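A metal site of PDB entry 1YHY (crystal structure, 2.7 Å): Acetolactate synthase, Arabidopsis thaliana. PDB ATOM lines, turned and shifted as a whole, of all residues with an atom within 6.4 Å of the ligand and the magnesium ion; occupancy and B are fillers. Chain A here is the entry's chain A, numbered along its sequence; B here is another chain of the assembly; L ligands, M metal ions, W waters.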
ATOM      1  N   GLY A 399      19.305  14.145  16.000  1.00  0.00           N
ATOM      2  CA  GLY A 399      18.517  13.199  16.756  1.00  0.00           C
ATOM      3  C   GLY A 399      17.909  12.315  15.695  1.00  0.00           C
ATOM      4  O   GLY A 399      18.477  12.152  14.614  1.00  0.00           O
ATOM      5  N   VAL A 400      16.735  11.757  15.982  1.00  0.00           N
ATOM      6  CA  VAL A 400      16.073  10.894  15.030  1.00  0.00           C
ATOM      7  C   VAL A 400      14.658  11.407  14.759  1.00  0.00           C
ATOM      8  O   VAL A 400      14.006  11.935  15.658  1.00  0.00           O
ATOM      9  CB  VAL A 400      16.009   9.448  15.562  1.00  0.00           C
ATOM     10  CG1 VAL A 400      15.099   8.603  14.684  1.00  0.00           C
ATOM     11  CG2 VAL A 400      17.415   8.869  15.618  1.00  0.00           C
ATOM     12  N   GLY A 401      14.196  11.265  13.519  1.00  0.00           N
ATOM     13  CA  GLY A 401      12.865  11.726  13.167  1.00  0.00           C
ATOM     14  C   GLY A 401      12.873  12.631  11.949  1.00  0.00           C
ATOM     15  O   GLY A 401      13.751  12.529  11.083  1.00  0.00           O
ATOM     16  N   GLN A 402      11.891  13.527  11.885  1.00  0.00           N
ATOM     17  CA  GLN A 402      11.769  14.453  10.763  1.00  0.00           C
ATOM     18  C   GLN A 402      12.954  15.394  10.670  1.00  0.00           C
ATOM     19  O   GLN A 402      13.537  15.565   9.606  1.00  0.00           O
ATOM     20  CB  GLN A 402      10.492  15.276  10.879  1.00  0.00           C
ATOM     21  CG  GLN A 402       9.213  14.470  10.830  1.00  0.00           C
ATOM     22  CD  GLN A 402       7.983  15.355  10.938  1.00  0.00           C
ATOM     23  OE1 GLN A 402       7.878  16.165  11.865  1.00  0.00           O
ATOM     24  NE2 GLN A 402       7.052  15.215   9.999  1.00  0.00           N
ATOM     25  N   HIS A 403      13.312  16.024  11.785  1.00  0.00           N
ATOM     26  CA  HIS A 403      14.432  16.955  11.772  1.00  0.00           C
ATOM     27  C   HIS A 403      15.683  16.270  11.225  1.00  0.00           C
ATOM     28  O   HIS A 403      16.484  16.887  10.510  1.00  0.00           O
ATOM     29  CB  HIS A 403      14.684  17.518  13.175  1.00  0.00           C
ATOM     30  CG  HIS A 403      15.222  16.521  14.147  1.00  0.00           C
ATOM     31  ND1 HIS A 403      16.564  16.356  14.391  1.00  0.00           N
ATOM     32  CD2 HIS A 403      14.583  15.629  14.943  1.00  0.00           C
ATOM     33  CE1 HIS A 403      16.729  15.411  15.298  1.00  0.00           C
ATOM     34  NE2 HIS A 403      15.547  14.956  15.659  1.00  0.00           N
ATOM     35  N   GLN A 404      15.834  14.984  11.540  1.00  0.00           N
ATOM     36  CA  GLN A 404      16.975  14.206  11.077  1.00  0.00           C
ATOM     37  C   GLN A 404      16.955  14.133   9.557  1.00  0.00           C
ATOM     38  O   GLN A 404      17.970  14.384   8.900  1.00  0.00           O
ATOM     39  CB  GLN A 404      16.898  12.792  11.666  1.00  0.00           C
ATOM     40  CG  GLN A 404      18.037  11.868  11.283  1.00  0.00           C
ATOM     41  CD  GLN A 404      17.776  10.443  11.701  1.00  0.00           C
ATOM     42  OE1 GLN A 404      18.692   9.630  11.793  1.00  0.00           O
ATOM     43  NE2 GLN A 404      16.506  10.127  11.974  1.00  0.00           N
ATOM     44  N   TRP A 406      15.422  16.142   7.441  1.00  0.00           N
ATOM     45  CA  TRP A 406      15.682  17.445   6.839  1.00  0.00           C
ATOM     46  C   TRP A 406      17.167  17.812   6.939  1.00  0.00           C
ATOM     47  O   TRP A 406      17.740  18.322   5.981  1.00  0.00           O
ATOM     48  CB  TRP A 406      14.806  18.537   7.474  1.00  0.00           C
ATOM     49  CG  TRP A 406      13.350  18.337   7.188  1.00  0.00           C
ATOM     50  CD1 TRP A 406      12.790  17.963   5.992  1.00  0.00           C
ATOM     51  CD2 TRP A 406      12.268  18.454   8.114  1.00  0.00           C
ATOM     52  NE1 TRP A 406      11.435  17.832   6.125  1.00  0.00           N
ATOM     53  CE2 TRP A 406      11.077  18.129   7.420  1.00  0.00           C
ATOM     54  CE3 TRP A 406      12.178  18.807   9.470  1.00  0.00           C
ATOM     55  CZ2 TRP A 406       9.817  18.142   8.031  1.00  0.00           C
ATOM     56  CZ3 TRP A 406      10.926  18.817  10.082  1.00  0.00           C
ATOM     57  CH2 TRP A 406       9.759  18.490   9.360  1.00  0.00           C
ATOM     58  N   MET A 428      17.008   7.865  19.512  1.00  0.00           N
ATOM     59  CA  MET A 428      16.747   9.245  19.917  1.00  0.00           C
ATOM     60  C   MET A 428      17.683   9.653  21.074  1.00  0.00           C
ATOM     61  O   MET A 428      18.107   8.817  21.875  1.00  0.00           O
ATOM     62  CB  MET A 428      15.295   9.391  20.368  1.00  0.00           C
ATOM     63  CG  MET A 428      14.289   9.475  19.217  1.00  0.00           C
ATOM     64  SD  MET A 428      12.593   9.432  19.831  1.00  0.00           S
ATOM     65  CE  MET A 428      12.526  10.966  20.743  1.00  0.00           C
ATOM     66  N   ASP A 451      18.730  19.114  16.484  1.00  0.00           N
ATOM     67  CA  ASP A 451      17.896  18.192  17.259  1.00  0.00           C
ATOM     68  C   ASP A 451      16.389  18.414  17.186  1.00  0.00           C
ATOM     69  O   ASP A 451      15.909  19.411  16.662  1.00  0.00           O
ATOM     70  CB  ASP A 451      18.333  18.267  18.719  1.00  0.00           C
ATOM     71  CG  ASP A 451      18.524  16.905  19.347  1.00  0.00           C
ATOM     72  OD1 ASP A 451      17.812  15.955  18.939  1.00  0.00           O
ATOM     73  OD2 ASP A 451      19.374  16.787  20.253  1.00  0.00           O
ATOM     74  N   GLY A 452      15.657  17.459  17.752  1.00  0.00           N
ATOM     75  CA  GLY A 452      14.212  17.543  17.804  1.00  0.00           C
ATOM     76  C   GLY A 452      13.873  17.785  19.257  1.00  0.00           C
ATOM     77  O   GLY A 452      14.685  17.489  20.136  1.00  0.00           O
ATOM     78  N   ASP A 453      12.690  18.318  19.552  1.00  0.00           N
ATOM     79  CA  ASP A 453      12.346  18.590  20.949  1.00  0.00           C
ATOM     80  C   ASP A 453      12.165  17.309  21.747  1.00  0.00           C
ATOM     81  O   ASP A 453      12.344  17.311  22.967  1.00  0.00           O
ATOM     82  CB  ASP A 453      11.082  19.468  21.049  1.00  0.00           C
ATOM     83  CG  ASP A 453       9.875  18.842  20.376  1.00  0.00           C
ATOM     84  OD1 ASP A 453       9.922  18.593  19.140  1.00  0.00           O
ATOM     85  OD2 ASP A 453       8.866  18.588  21.075  1.00  0.00           O
ATOM     86  N   GLY A 454      11.830  16.216  21.072  1.00  0.00           N
ATOM     87  CA  GLY A 454      11.655  14.955  21.762  1.00  0.00           C
ATOM     88  C   GLY A 454      12.984  14.285  22.034  1.00  0.00           C
ATOM     89  O   GLY A 454      13.227  13.785  23.139  1.00  0.00           O
ATOM     90  N   SER A 455      13.857  14.274  21.021  1.00  0.00           N
ATOM     91  CA  SER A 455      15.170  13.668  21.138  1.00  0.00           C
ATOM     92  C   SER A 455      16.066  14.484  22.059  1.00  0.00           C
ATOM     93  O   SER A 455      16.814  13.936  22.859  1.00  0.00           O
ATOM     94  CB  SER A 455      15.832  13.567  19.765  1.00  0.00           C
ATOM     95  OG  SER A 455      15.079  12.739  18.889  1.00  0.00           O
ATOM     96  N   PHE A 456      15.981  15.811  21.931  1.00  0.00           N
ATOM     97  CA  PHE A 456      16.812  16.686  22.739  1.00  0.00           C
ATOM     98  C   PHE A 456      16.614  16.460  24.235  1.00  0.00           C
ATOM     99  O   PHE A 456      17.586  16.317  24.991  1.00  0.00           O
ATOM    100  CB  PHE A 456      16.505  18.145  22.415  1.00  0.00           C
ATOM    101  CG  PHE A 456      17.352  19.127  23.177  1.00  0.00           C
ATOM    102  CD1 PHE A 456      18.699  19.306  22.855  1.00  0.00           C
ATOM    103  CD2 PHE A 456      16.817  19.845  24.256  1.00  0.00           C
ATOM    104  CE1 PHE A 456      19.495  20.184  23.584  1.00  0.00           C
ATOM    105  CE2 PHE A 456      17.625  20.728  24.988  1.00  0.00           C
ATOM    106  CZ  PHE A 456      18.958  20.895  24.651  1.00  0.00           C
ATOM    107  N   LEU A 478      14.966  22.167  16.427  1.00  0.00           N
ATOM    108  CA  LEU A 478      13.768  22.380  15.615  1.00  0.00           C
ATOM    109  C   LEU A 478      12.595  21.918  16.476  1.00  0.00           C
ATOM    110  O   LEU A 478      12.222  20.742  16.463  1.00  0.00           O
ATOM    111  CB  LEU A 478      13.862  21.573  14.322  1.00  0.00           C
ATOM    112  CG  LEU A 478      15.128  21.821  13.502  1.00  0.00           C
ATOM    113  CD1 LEU A 478      15.072  21.017  12.204  1.00  0.00           C
ATOM    114  CD2 LEU A 478      15.272  23.301  13.200  1.00  0.00           C
ATOM    115  N   ASN A 479      12.014  22.853  17.222  1.00  0.00           N
ATOM    116  CA  ASN A 479      10.912  22.549  18.132  1.00  0.00           C
ATOM    117  C   ASN A 479       9.536  22.542  17.467  1.00  0.00           C
ATOM    118  O   ASN A 479       9.056  23.576  17.003  1.00  0.00           O
ATOM    119  CB  ASN A 479      10.913  23.579  19.263  1.00  0.00           C
ATOM    120  CG  ASN A 479      10.201  23.080  20.511  1.00  0.00           C
ATOM    121  OD1 ASN A 479       9.227  22.324  20.423  1.00  0.00           O
ATOM    122  ND2 ASN A 479      10.672  23.520  21.675  1.00  0.00           N
ATOM    123  N   ASN A 480       8.904  21.362  17.427  1.00  0.00           N
ATOM    124  CA  ASN A 480       7.587  21.225  16.826  1.00  0.00           C
ATOM    125  C   ASN A 480       6.579  20.608  17.806  1.00  0.00           C
ATOM    126  O   ASN A 480       5.501  20.142  17.402  1.00  0.00           O
ATOM    127  CB  ASN A 480       7.671  20.371  15.552  1.00  0.00           C
ATOM    128  CG  ASN A 480       7.938  18.913  15.848  1.00  0.00           C
ATOM    129  OD1 ASN A 480       8.376  18.542  16.936  1.00  0.00           O
ATOM    130  ND2 ASN A 480       7.665  18.068  14.856  1.00  0.00           N
ATOM    131  N   GLN A 481       6.924  20.605  19.086  1.00  0.00           N
ATOM    132  CA  GLN A 481       6.058  20.088  20.145  1.00  0.00           C
ATOM    133  C   GLN A 481       5.517  18.675  19.953  1.00  0.00           C
ATOM    134  O   GLN A 481       4.639  18.245  20.697  1.00  0.00           O
ATOM    135  CB  GLN A 481       4.879  21.037  20.349  1.00  0.00           C
ATOM    136  CG  GLN A 481       5.248  22.463  20.721  1.00  0.00           C
ATOM    137  CD  GLN A 481       5.901  22.571  22.092  1.00  0.00           C
ATOM    138  OE1 GLN A 481       7.092  22.285  22.261  1.00  0.00           O
ATOM    139  NE2 GLN A 481       5.115  22.977  23.086  1.00  0.00           N
ATOM    140  N   HIS A 482       6.024  17.956  18.952  1.00  0.00           N
ATOM    141  CA  HIS A 482       5.545  16.597  18.680  1.00  0.00           C
ATOM    142  C   HIS A 482       6.655  15.593  18.378  1.00  0.00           C
ATOM    143  O   HIS A 482       7.809  15.953  18.146  1.00  0.00           O
ATOM    144  CB  HIS A 482       4.615  16.561  17.463  1.00  0.00           C
ATOM    145  CG  HIS A 482       3.267  17.155  17.691  1.00  0.00           C
ATOM    146  ND1 HIS A 482       3.060  18.510  17.851  1.00  0.00           N
ATOM    147  CD2 HIS A 482       2.039  16.577  17.745  1.00  0.00           C
ATOM    148  CE1 HIS A 482       1.765  18.735  17.983  1.00  0.00           C
ATOM    149  NE2 HIS A 482       1.125  17.585  17.927  1.00  0.00           N
ATOM    150  N   LEU A 483       6.276  14.325  18.384  1.00  0.00           N
ATOM    151  CA  LEU A 483       7.194  13.260  18.012  1.00  0.00           C
ATOM    152  C   LEU A 483       6.922  13.211  16.515  1.00  0.00           C
ATOM    153  O   LEU A 483       6.185  12.365  16.012  1.00  0.00           O
ATOM    154  CB  LEU A 483       6.802  11.941  18.691  1.00  0.00           C
ATOM    155  CG  LEU A 483       7.177  11.868  20.169  1.00  0.00           C
ATOM    156  CD1 LEU A 483       6.708  10.556  20.773  1.00  0.00           C
ATOM    157  CD2 LEU A 483       8.687  12.011  20.316  1.00  0.00           C
ATOM    158  N   GLY A 484       7.518  14.178  15.823  1.00  0.00           N
ATOM    159  CA  GLY A 484       7.360  14.342  14.395  1.00  0.00           C
ATOM    160  C   GLY A 484       7.149  13.180  13.455  1.00  0.00           C
ATOM    161  O   GLY A 484       6.089  13.058  12.842  1.00  0.00           O
ATOM    162  N   MET A 485       8.163  12.320  13.315  1.00  0.00           N
ATOM    163  CA  MET A 485       8.055  11.202  12.394  1.00  0.00           C
ATOM    164  C   MET A 485       6.871  10.284  12.710  1.00  0.00           C
ATOM    165  O   MET A 485       6.219   9.772  11.799  1.00  0.00           O
ATOM    166  CB  MET A 485       9.352  10.392  12.357  1.00  0.00           C
ATOM    167  CG  MET A 485       9.398   9.372  11.246  1.00  0.00           C
ATOM    168  SD  MET A 485       9.027  10.086   9.625  1.00  0.00           S
ATOM    169  CE  MET A 485      10.632  10.678   9.152  1.00  0.00           C
ATOM    170  N   VAL A 486       6.590  10.075  13.997  1.00  0.00           N
ATOM    171  CA  VAL A 486       5.471   9.213  14.339  1.00  0.00           C
ATOM    172  C   VAL A 486       4.133   9.882  14.044  1.00  0.00           C
ATOM    173  O   VAL A 486       3.186   9.208  13.647  1.00  0.00           O
ATOM    174  CB  VAL A 486       5.511   8.800  15.824  1.00  0.00           C
ATOM    175  CG1 VAL A 486       4.355   7.865  16.121  1.00  0.00           C
ATOM    176  CG2 VAL A 486       6.811   8.092  16.113  1.00  0.00           C
ATOM    177  N   MET A 487       4.045  11.212  14.208  1.00  0.00           N
ATOM    178  CA  MET A 487       2.793  11.879  13.918  1.00  0.00           C
ATOM    179  C   MET A 487       2.581  11.921  12.411  1.00  0.00           C
ATOM    180  O   MET A 487       1.436  11.966  11.945  1.00  0.00           O
ATOM    181  CB  MET A 487       2.730  13.300  14.493  1.00  0.00           C
ATOM    182  CG  MET A 487       3.601  14.300  13.785  1.00  0.00           C
ATOM    183  SD  MET A 487       2.757  15.871  13.556  1.00  0.00           S
ATOM    184  CE  MET A 487       2.910  16.031  11.777  1.00  0.00           C
ATOM    185  N   LEU A 503       4.127  16.345  22.659  1.00  0.00           N
ATOM    186  CA  LEU A 503       5.069  16.521  23.764  1.00  0.00           C
ATOM    187  C   LEU A 503       4.861  17.754  24.634  1.00  0.00           C
ATOM    188  O   LEU A 503       5.592  17.965  25.594  1.00  0.00           O
ATOM    189  CB  LEU A 503       6.505  16.528  23.231  1.00  0.00           C
ATOM    190  CG  LEU A 503       6.953  15.268  22.481  1.00  0.00           C
ATOM    191  CD1 LEU A 503       8.275  15.547  21.782  1.00  0.00           C
ATOM    192  CD2 LEU A 503       7.072  14.091  23.440  1.00  0.00           C
ATOM    193  N   TYR B  33       5.962   4.697  25.535  1.00  0.00           N
ATOM    194  CA  TYR B  33       6.555   5.733  24.691  1.00  0.00           C
ATOM    195  C   TYR B  33       6.437   5.226  23.262  1.00  0.00           C
ATOM    196  O   TYR B  33       7.072   4.237  22.889  1.00  0.00           O
ATOM    197  CB  TYR B  33       8.010   5.945  25.052  1.00  0.00           C
ATOM    198  CG  TYR B  33       8.598   7.210  24.490  1.00  0.00           C
ATOM    199  CD1 TYR B  33       8.561   8.404  25.194  1.00  0.00           C
ATOM    200  CD2 TYR B  33       9.193   7.211  23.232  1.00  0.00           C
ATOM    201  CE1 TYR B  33       9.088   9.583  24.663  1.00  0.00           C
ATOM    202  CE2 TYR B  33       9.729   8.379  22.690  1.00  0.00           C
ATOM    203  CZ  TYR B  33       9.672   9.555  23.408  1.00  0.00           C
ATOM    204  OH  TYR B  33      10.208  10.699  22.870  1.00  0.00           O
HETATM  205  C1  LIG L   1       9.690  11.162  16.166  1.00  0.00           C
HETATM  206  C2  LIG L   1      10.702  11.846  17.119  1.00  0.00           C
HETATM  207  O1  LIG L   1      10.723  13.004  17.982  1.00  0.00           O
HETATM  208  P1  LIG L   1      11.634  14.330  17.730  1.00  0.00           P
HETATM  209  O2  LIG L   1      10.999  15.472  18.336  1.00  0.00           O
HETATM  210  O3  LIG L   1      12.918  14.172  18.320  1.00  0.00           O
HETATM  211  O4  LIG L   1      11.823  14.712  16.206  1.00  0.00           O
HETATM  212  P2  LIG L   1      10.888  15.029  14.966  1.00  0.00           P
HETATM  213  O5  LIG L   1      10.570  13.750  14.334  1.00  0.00           O
HETATM  214  O6  LIG L   1      11.723  15.927  14.196  1.00  0.00           O
HETATM  215  O7  LIG L   1       9.768  15.736  15.604  1.00  0.00           O
HETATM  216 MG    MG M   1       9.695  16.749  17.521  1.00  0.00          MG
HETATM  217  O   HOH W   1      11.253  18.323  16.463  1.00  0.00           O
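O3 of the ligand lies within hydrogen-bond range of N of Ser 455 (2.9 Å). O3 of the ligand sits at hydrogen-bond distance from OG of Ser 455 (2.7 Å). N of Gly 484 sits close to O5 of the ligand, at 3.4 Å. N of Gln 402 sits at hydrogen-bond distance from O5 of the ligand, 2.8 Å away. N of His 403 sits at hydrogen-bond distance from O6 of the ligand. O2 of the ligand sits close to N of Gly 454 (3.0 Å). The backbone NH (N) of Met 485 lies within hydrogen-bond range of an oxygen (O5) of the ligand (3.0 Å).
The side-chain carboxylate of Asp 453 lies close to the backbone NH of Gln 481 (3.4 Å). The side-chain hydroxyl of Ser 455 sits at hydrogen-bond distance from the backbone NH of Val 400, at 3.5 Å. A ring nitrogen (NE2) of His 403 is in hydrogen-bond range of the backbone carbonyl oxygen (O) of Val 400, 3.4 Å away. A ring nitrogen (NE2) of His 403 lies within hydrogen-bond range of the backbone NH (N) of Gly 452. N of Gly 401 lies close to NE2 of Gln 404 (3.0 Å).
Residues that only touch the ligand: Val 400 (3.6 Å), Gly 401 (3.3 Å), Met 428 (3.9 Å), Gly 452 (3.6 Å), Leu 483 (3.3 Å) and Val 486 (3.9 Å). Hydrophobic or aromatic side chains within 4 Å of the ligand: His 403, Met 428, Leu 483 and Met 485. 15 residues have an atom within 4 Å of the ligand: Val 400, Gly 401, Gln 402, His 403, Met 428, Gly 452, Asp 453, Gly 454, Ser 455, Asn 480, His 482, Leu 483, Gly 484, Met 485 and Val 486. The nearest printed residue that does not touch the ligand is Leu 503 (4.4 Å).
Merely in contact with the magnesium ion: Gly 484. Along chain A the residues within 4 Å of the magnesium ion span positions 453 to 484. The nearest printed residue that does not touch the magnesium ion is Gly 454 (4.2 Å).
The magnesium ion is bound by O2 of the ligand, O of His 482, O7 of the ligand, OD1 of Asn 480, water W1 and OD1 of Asp 453.
Water W1 lies within hydrogen-bond range of O of Leu 478 (2.6 Å), O6 of the ligand (3.3 Å) and N of Asp 453 (3.4 Å).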
